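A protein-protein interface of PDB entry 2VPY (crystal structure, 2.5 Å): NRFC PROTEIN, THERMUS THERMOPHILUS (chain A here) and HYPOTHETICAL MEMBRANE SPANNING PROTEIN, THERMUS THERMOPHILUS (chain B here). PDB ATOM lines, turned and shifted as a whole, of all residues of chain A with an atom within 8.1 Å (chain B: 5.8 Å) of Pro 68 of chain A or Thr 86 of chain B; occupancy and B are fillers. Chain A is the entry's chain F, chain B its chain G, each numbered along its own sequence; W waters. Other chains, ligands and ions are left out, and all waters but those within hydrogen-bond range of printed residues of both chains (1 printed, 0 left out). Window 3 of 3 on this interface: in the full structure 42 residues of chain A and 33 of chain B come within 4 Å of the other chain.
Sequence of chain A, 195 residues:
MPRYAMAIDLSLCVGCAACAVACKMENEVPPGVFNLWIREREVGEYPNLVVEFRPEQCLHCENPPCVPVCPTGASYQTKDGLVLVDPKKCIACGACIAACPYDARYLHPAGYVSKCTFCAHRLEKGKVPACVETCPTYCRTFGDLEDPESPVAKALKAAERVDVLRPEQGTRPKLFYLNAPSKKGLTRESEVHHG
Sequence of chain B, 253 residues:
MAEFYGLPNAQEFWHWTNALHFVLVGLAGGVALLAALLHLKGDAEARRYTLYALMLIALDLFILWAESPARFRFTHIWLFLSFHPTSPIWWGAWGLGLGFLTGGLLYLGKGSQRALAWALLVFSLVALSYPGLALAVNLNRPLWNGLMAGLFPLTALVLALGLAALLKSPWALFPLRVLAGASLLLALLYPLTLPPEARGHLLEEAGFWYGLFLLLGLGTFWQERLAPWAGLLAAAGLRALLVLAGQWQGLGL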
ATOM      1  N   ASN A  63       8.700  -4.743 -38.090  1.00  0.00           N
ATOM      2  CA  ASN A  63       8.994  -5.984 -37.418  1.00  0.00           C
ATOM      3  C   ASN A  63       9.302  -5.512 -35.992  1.00  0.00           C
ATOM      4  O   ASN A  63      10.417  -5.666 -35.486  1.00  0.00           O
ATOM      5  CB  ASN A  63      10.190  -6.584 -38.147  1.00  0.00           C
ATOM      6  CG  ASN A  63      10.738  -7.782 -37.482  1.00  0.00           C
ATOM      7  OD1 ASN A  63      10.020  -8.742 -37.220  1.00  0.00           O
ATOM      8  ND2 ASN A  63      12.024  -7.744 -37.181  1.00  0.00           N
ATOM      9  N   PRO A  64       8.264  -4.975 -35.308  1.00  0.00           N
ATOM     10  CA  PRO A  64       8.363  -4.444 -33.951  1.00  0.00           C
ATOM     11  C   PRO A  64       8.708  -5.290 -32.764  1.00  0.00           C
ATOM     12  O   PRO A  64       7.926  -6.124 -32.338  1.00  0.00           O
ATOM     13  CB  PRO A  64       7.034  -3.730 -33.753  1.00  0.00           C
ATOM     14  CG  PRO A  64       6.071  -4.562 -34.508  1.00  0.00           C
ATOM     15  CD  PRO A  64       6.848  -5.233 -35.645  1.00  0.00           C
ATOM     16  N   PRO A  65       9.864  -5.009 -32.151  1.00  0.00           N
ATOM     17  CA  PRO A  65      10.152  -5.857 -31.004  1.00  0.00           C
ATOM     18  C   PRO A  65       9.214  -5.720 -29.791  1.00  0.00           C
ATOM     19  O   PRO A  65       9.200  -6.596 -28.920  1.00  0.00           O
ATOM     20  CB  PRO A  65      11.611  -5.526 -30.658  1.00  0.00           C
ATOM     21  CG  PRO A  65      11.890  -4.198 -31.292  1.00  0.00           C
ATOM     22  CD  PRO A  65      10.852  -3.929 -32.336  1.00  0.00           C
ATOM     23  N   CYS A  66       8.419  -4.651 -29.745  1.00  0.00           N
ATOM     24  CA  CYS A  66       7.512  -4.364 -28.615  1.00  0.00           C
ATOM     25  C   CYS A  66       6.178  -5.127 -28.554  1.00  0.00           C
ATOM     26  O   CYS A  66       5.511  -5.157 -27.503  1.00  0.00           O
ATOM     27  CB  CYS A  66       7.222  -2.861 -28.564  1.00  0.00           C
ATOM     28  SG  CYS A  66       6.551  -2.247 -30.090  1.00  0.00           S
ATOM     29  N   VAL A  67       5.803  -5.718 -29.687  1.00  0.00           N
ATOM     30  CA  VAL A  67       4.589  -6.516 -29.858  1.00  0.00           C
ATOM     31  C   VAL A  67       4.772  -7.942 -29.238  1.00  0.00           C
ATOM     32  O   VAL A  67       4.078  -8.267 -28.262  1.00  0.00           O
ATOM     33  CB  VAL A  67       4.180  -6.593 -31.396  1.00  0.00           C
ATOM     34  CG1 VAL A  67       3.121  -7.646 -31.617  1.00  0.00           C
ATOM     35  CG2 VAL A  67       3.646  -5.241 -31.897  1.00  0.00           C
ATOM     36  N   PRO A  68       5.710  -8.792 -29.761  1.00  0.00           N
ATOM     37  CA  PRO A  68       5.991 -10.164 -29.276  1.00  0.00           C
ATOM     38  C   PRO A  68       6.227 -10.376 -27.781  1.00  0.00           C
ATOM     39  O   PRO A  68       6.043 -11.461 -27.213  1.00  0.00           O
ATOM     40  CB  PRO A  68       7.258 -10.544 -30.035  1.00  0.00           C
ATOM     41  CG  PRO A  68       7.024  -9.962 -31.357  1.00  0.00           C
ATOM     42  CD  PRO A  68       6.461  -8.558 -31.011  1.00  0.00           C
ATOM     43  N   VAL A  69       6.651  -9.304 -27.170  1.00  0.00           N
ATOM     44  CA  VAL A  69       7.072  -9.249 -25.795  1.00  0.00           C
ATOM     45  C   VAL A  69       5.927  -9.053 -24.773  1.00  0.00           C
ATOM     46  O   VAL A  69       6.046  -9.361 -23.579  1.00  0.00           O
ATOM     47  CB  VAL A  69       8.141  -8.122 -25.823  1.00  0.00           C
ATOM     48  CG1 VAL A  69       7.616  -6.867 -25.175  1.00  0.00           C
ATOM     49  CG2 VAL A  69       9.466  -8.629 -25.333  1.00  0.00           C
ATOM     50  N   CYS A  70       4.806  -8.570 -25.300  1.00  0.00           N
ATOM     51  CA  CYS A  70       3.581  -8.287 -24.555  1.00  0.00           C
ATOM     52  C   CYS A  70       2.862  -9.581 -24.123  1.00  0.00           C
ATOM     53  O   CYS A  70       2.572 -10.433 -24.957  1.00  0.00           O
ATOM     54  CB  CYS A  70       2.651  -7.433 -25.437  1.00  0.00           C
ATOM     55  SG  CYS A  70       1.145  -6.745 -24.617  1.00  0.00           S
ATOM     56  N   PRO A  71       2.566  -9.741 -22.812  1.00  0.00           N
ATOM     57  CA  PRO A  71       1.877 -10.959 -22.355  1.00  0.00           C
ATOM     58  C   PRO A  71       0.360 -10.939 -22.561  1.00  0.00           C
ATOM     59  O   PRO A  71      -0.298 -11.961 -22.796  1.00  0.00           O
ATOM     60  CB  PRO A  71       2.232 -11.045 -20.875  1.00  0.00           C
ATOM     61  CG  PRO A  71       2.554  -9.605 -20.451  1.00  0.00           C
ATOM     62  CD  PRO A  71       2.778  -8.782 -21.709  1.00  0.00           C
ATOM     63  N   THR A  72      -0.157  -9.738 -22.489  1.00  0.00           N
ATOM     64  CA  THR A  72      -1.549  -9.472 -22.601  1.00  0.00           C
ATOM     65  C   THR A  72      -2.148  -9.469 -24.013  1.00  0.00           C
ATOM     66  O   THR A  72      -3.262  -9.955 -24.211  1.00  0.00           O
ATOM     67  CB  THR A  72      -1.760  -8.144 -21.900  1.00  0.00           C
ATOM     68  OG1 THR A  72      -2.392  -8.365 -20.642  1.00  0.00           O
ATOM     69  CG2 THR A  72      -2.510  -7.201 -22.778  1.00  0.00           C
ATOM     70  N   SER A  75      -0.479  -4.844 -27.095  1.00  0.00           N
ATOM     71  CA  SER A  75       0.494  -4.316 -28.048  1.00  0.00           C
ATOM     72  C   SER A  75       0.244  -5.135 -29.305  1.00  0.00           C
ATOM     73  O   SER A  75       0.582  -6.309 -29.334  1.00  0.00           O
ATOM     74  CB  SER A  75       1.906  -4.580 -27.511  1.00  0.00           C
ATOM     75  OG  SER A  75       2.908  -3.887 -28.225  1.00  0.00           O
ATOM     76  N   TYR A  76      -0.340  -4.539 -30.334  1.00  0.00           N
ATOM     77  CA  TYR A  76      -0.653  -5.295 -31.537  1.00  0.00           C
ATOM     78  C   TYR A  76      -0.216  -4.522 -32.753  1.00  0.00           C
ATOM     79  O   TYR A  76      -0.065  -3.312 -32.687  1.00  0.00           O
ATOM     80  CB  TYR A  76      -2.166  -5.577 -31.583  1.00  0.00           C
ATOM     81  CG  TYR A  76      -3.067  -4.342 -31.621  1.00  0.00           C
ATOM     82  CD1 TYR A  76      -3.593  -3.871 -32.835  1.00  0.00           C
ATOM     83  CD2 TYR A  76      -3.429  -3.669 -30.443  1.00  0.00           C
ATOM     84  CE1 TYR A  76      -4.466  -2.765 -32.876  1.00  0.00           C
ATOM     85  CE2 TYR A  76      -4.306  -2.556 -30.472  1.00  0.00           C
ATOM     86  CZ  TYR A  76      -4.822  -2.115 -31.690  1.00  0.00           C
ATOM     87  OH  TYR A  76      -5.702  -1.052 -31.734  1.00  0.00           O
ATOM     88  N   GLN A  77      -0.002  -5.219 -33.854  1.00  0.00           N
ATOM     89  CA  GLN A  77       0.421  -4.576 -35.079  1.00  0.00           C
ATOM     90  C   GLN A  77      -0.767  -4.745 -36.014  1.00  0.00           C
ATOM     91  O   GLN A  77      -1.303  -5.834 -36.180  1.00  0.00           O
ATOM     92  CB  GLN A  77       1.689  -5.253 -35.588  1.00  0.00           C
ATOM     93  CG  GLN A  77       2.309  -4.643 -36.816  1.00  0.00           C
ATOM     94  CD  GLN A  77       3.457  -5.482 -37.363  1.00  0.00           C
ATOM     95  OE1 GLN A  77       4.117  -5.094 -38.332  1.00  0.00           O
ATOM     96  NE2 GLN A  77       3.697  -6.637 -36.750  1.00  0.00           N
ATOM     97  N   VAL A  83       1.598   0.347 -35.027  1.00  0.00           N
ATOM     98  CA  VAL A  83       1.760  -0.397 -33.797  1.00  0.00           C
ATOM     99  C   VAL A  83       0.930   0.482 -32.848  1.00  0.00           C
ATOM    100  O   VAL A  83       1.109   1.697 -32.789  1.00  0.00           O
ATOM    101  CB  VAL A  83       3.266  -0.519 -33.382  1.00  0.00           C
ATOM    102  CG1 VAL A  83       3.423  -1.371 -32.101  1.00  0.00           C
ATOM    103  CG2 VAL A  83       4.038  -1.184 -34.520  1.00  0.00           C
ATOM    104  N   ALA A  95       7.239  -4.430 -20.451  1.00  0.00           N
ATOM    105  CA  ALA A  95       8.059  -5.289 -21.306  1.00  0.00           C
ATOM    106  C   ALA A  95       8.362  -4.679 -22.667  1.00  0.00           C
ATOM    107  O   ALA A  95       9.454  -4.865 -23.212  1.00  0.00           O
ATOM    108  CB  ALA A  95       7.422  -6.687 -21.481  1.00  0.00           C
ATOM    109  N   CYS A  96       7.386  -3.940 -23.187  1.00  0.00           N
ATOM    110  CA  CYS A  96       7.465  -3.273 -24.476  1.00  0.00           C
ATOM    111  C   CYS A  96       8.447  -2.093 -24.418  1.00  0.00           C
ATOM    112  O   CYS A  96       9.158  -1.828 -25.390  1.00  0.00           O
ATOM    113  CB  CYS A  96       6.064  -2.821 -24.907  1.00  0.00           C
ATOM    114  SG  CYS A  96       5.157  -1.821 -23.626  1.00  0.00           S
ATOM    115  N   ALA A  99      11.782  -3.600 -24.628  1.00  0.00           N
ATOM    116  CA  ALA A  99      12.084  -4.069 -25.975  1.00  0.00           C
ATOM    117  C   ALA A  99      12.108  -2.978 -27.074  1.00  0.00           C
ATOM    118  O   ALA A  99      12.569  -3.236 -28.185  1.00  0.00           O
ATOM    119  CB  ALA A  99      11.100  -5.214 -26.359  1.00  0.00           C
ATOM    120  N   HIS B  84       0.185 -16.363 -25.649  1.00  0.00           N
ATOM    121  CA  HIS B  84       1.320 -15.524 -26.064  1.00  0.00           C
ATOM    122  C   HIS B  84       2.686 -16.101 -25.717  1.00  0.00           C
ATOM    123  O   HIS B  84       3.435 -15.513 -24.925  1.00  0.00           O
ATOM    124  CB  HIS B  84       1.212 -14.116 -25.454  1.00  0.00           C
ATOM    125  CG  HIS B  84       0.025 -13.340 -25.918  1.00  0.00           C
ATOM    126  ND1 HIS B  84      -0.102 -12.863 -27.198  1.00  0.00           N
ATOM    127  CD2 HIS B  84      -1.116 -13.011 -25.284  1.00  0.00           C
ATOM    128  CE1 HIS B  84      -1.275 -12.279 -27.337  1.00  0.00           C
ATOM    129  NE2 HIS B  84      -1.912 -12.356 -26.188  1.00  0.00           N
ATOM    130  N   PRO B  85       3.014 -17.263 -26.312  1.00  0.00           N
ATOM    131  CA  PRO B  85       4.235 -18.069 -26.200  1.00  0.00           C
ATOM    132  C   PRO B  85       5.563 -17.321 -26.448  1.00  0.00           C
ATOM    133  O   PRO B  85       6.618 -17.772 -26.004  1.00  0.00           O
ATOM    134  CB  PRO B  85       4.005 -19.188 -27.217  1.00  0.00           C
ATOM    135  CG  PRO B  85       3.011 -18.573 -28.205  1.00  0.00           C
ATOM    136  CD  PRO B  85       2.079 -17.886 -27.260  1.00  0.00           C
ATOM    137  N   THR B  86       5.518 -16.198 -27.160  1.00  0.00           N
ATOM    138  CA  THR B  86       6.723 -15.408 -27.451  1.00  0.00           C
ATOM    139  C   THR B  86       7.140 -14.504 -26.298  1.00  0.00           C
ATOM    140  O   THR B  86       8.220 -13.918 -26.315  1.00  0.00           O
ATOM    141  CB  THR B  86       6.527 -14.443 -28.671  1.00  0.00           C
ATOM    142  OG1 THR B  86       5.284 -13.744 -28.546  1.00  0.00           O
ATOM    143  CG2 THR B  86       6.584 -15.200 -29.980  1.00  0.00           C
ATOM    144  N   SER B  87       6.297 -14.428 -25.286  1.00  0.00           N
ATOM    145  CA  SER B  87       6.485 -13.504 -24.166  1.00  0.00           C
ATOM    146  C   SER B  87       7.028 -14.021 -22.834  1.00  0.00           C
ATOM    147  O   SER B  87       6.271 -14.586 -22.055  1.00  0.00           O
ATOM    148  CB  SER B  87       5.121 -12.805 -23.962  1.00  0.00           C
ATOM    149  OG  SER B  87       5.028 -12.037 -22.779  1.00  0.00           O
ATOM    150  N   PRO B  88       8.332 -13.819 -22.533  1.00  0.00           N
ATOM    151  CA  PRO B  88       8.794 -14.337 -21.239  1.00  0.00           C
ATOM    152  C   PRO B  88       7.812 -14.161 -20.065  1.00  0.00           C
ATOM    153  O   PRO B  88       7.517 -15.115 -19.357  1.00  0.00           O
ATOM    154  CB  PRO B  88      10.100 -13.584 -20.996  1.00  0.00           C
ATOM    155  CG  PRO B  88      10.656 -13.422 -22.361  1.00  0.00           C
ATOM    156  CD  PRO B  88       9.437 -13.181 -23.268  1.00  0.00           C
ATOM    157  N   TRP B  91       4.756 -16.547 -19.983  1.00  0.00           N
ATOM    158  CA  TRP B  91       5.203 -17.868 -19.518  1.00  0.00           C
ATOM    159  C   TRP B  91       5.388 -17.935 -17.998  1.00  0.00           C
ATOM    160  O   TRP B  91       5.350 -19.018 -17.414  1.00  0.00           O
ATOM    161  CB  TRP B  91       6.543 -18.275 -20.146  1.00  0.00           C
ATOM    162  CG  TRP B  91       6.452 -18.862 -21.503  1.00  0.00           C
ATOM    163  CD1 TRP B  91       6.518 -18.197 -22.691  1.00  0.00           C
ATOM    164  CD2 TRP B  91       6.259 -20.241 -21.822  1.00  0.00           C
ATOM    165  NE1 TRP B  91       6.380 -19.079 -23.731  1.00  0.00           N
ATOM    166  CE2 TRP B  91       6.218 -20.341 -23.228  1.00  0.00           C
ATOM    167  CE3 TRP B  91       6.113 -21.406 -21.053  1.00  0.00           C
ATOM    168  CZ2 TRP B  91       6.037 -21.565 -23.892  1.00  0.00           C
ATOM    169  CZ3 TRP B  91       5.932 -22.628 -21.707  1.00  0.00           C
ATOM    170  CH2 TRP B  91       5.896 -22.693 -23.118  1.00  0.00           C
ATOM    171  N   VAL B 137      15.726 -11.014 -23.703  1.00  0.00           N
ATOM    172  CA  VAL B 137      14.975 -10.989 -24.924  1.00  0.00           C
ATOM    173  C   VAL B 137      15.111  -9.630 -25.625  1.00  0.00           C
ATOM    174  O   VAL B 137      14.921  -9.532 -26.840  1.00  0.00           O
ATOM    175  CB  VAL B 137      13.496 -11.325 -24.647  1.00  0.00           C
ATOM    176  CG1 VAL B 137      12.681 -10.064 -24.395  1.00  0.00           C
ATOM    177  CG2 VAL B 137      12.952 -12.104 -25.792  1.00  0.00           C
HETATM  178  O   HOH W   1       2.134 -10.530 -27.823  1.00  0.00           O
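The backbone carbonyl oxygen (O) of Pro 68 of chain A is in hydrogen-bond range of the side-chain hydroxyl (OG1) of Thr 86 of chain B, at 2.8 Å.
The backbone carbonyl oxygen (O) of Val 69 of chain A lies within hydrogen-bond range of the side-chain hydroxyl (OG) of Ser 87 of chain B (3.0 Å).
The backbone carbonyl oxygen of Thr 72 of chain A sits at hydrogen-bond distance from a ring nitrogen (NE2) of His 84 of chain B.
N of Pro 71 of chain A sits close to OG of Ser 87 of chain B, 3.4 Å away.
SG of Cys 70 of chain A lies close to N of Ser 75 of chain A (3.5 Å).
Among the printed residues, pairs that only touch across the chains: Pro 68 of chain A with Ser 87 of chain B (3.5 Å), Val 69 of chain A with Val 137 of chain B (3.6 Å), Cys 70 of chain A with His 84 of chain B (3.96 Å), Cys 70 of chain A with Ser 87 of chain B (3.5 Å) and Pro 71 of chain A with His 84 of chain B (2.8 Å).
Of the printed residues of chain B, Pro 68 of chain A touches Thr 86 (2.8 Å) and Ser 87 (3.5 Å).
Of the printed residues of chain A, Thr 86 of chain B touches Pro 68.
No residue of chain A comes within 4 Å of Pro 85 of chain B.
Of the printed residues of chain B, Thr 72 of chain A touches His 84.
Printed residues of chain A within 4 Å of Val 137 of chain B: Val 69 (3.6 Å).
Printed residues of chain A within 4 Å of His 84 of chain B: Cys 70, Pro 71 and Thr 72.
Pro 64 of chain A touches none of the printed residues of chain B.
Ala 95 of chain A touches none of the printed residues of chain B.
The nearest residue of chain B that does not touch Pro 68 of chain A is His 84 of chain B (5.3 Å).
The nearest residue of chain A that does not touch Thr 86 of chain B is Val 69 of chain A (4.8 Å).
The nearest printed residue of chain A that does not touch Val 137 of chain B is Ala 99 of chain A (5.5 Å).
Hydrophobic or aromatic side chains of chain B that line the printed part of chain A: His 84 and Val 137.
Of the 17 printed residues of chain A, 5 touch a printed residue of chain B.
Among the printed residues, 9 pairs touch across the chains.
Among the printed residues, no Asp or Glu carboxylate lies within 4 Å of a Lys or Arg side-chain nitrogen of the other chain.
Water W1 lies within hydrogen-bond range of O of Cys 70 of chain A, O of Val 67 of chain A and ND1 of His 84 of chain B.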
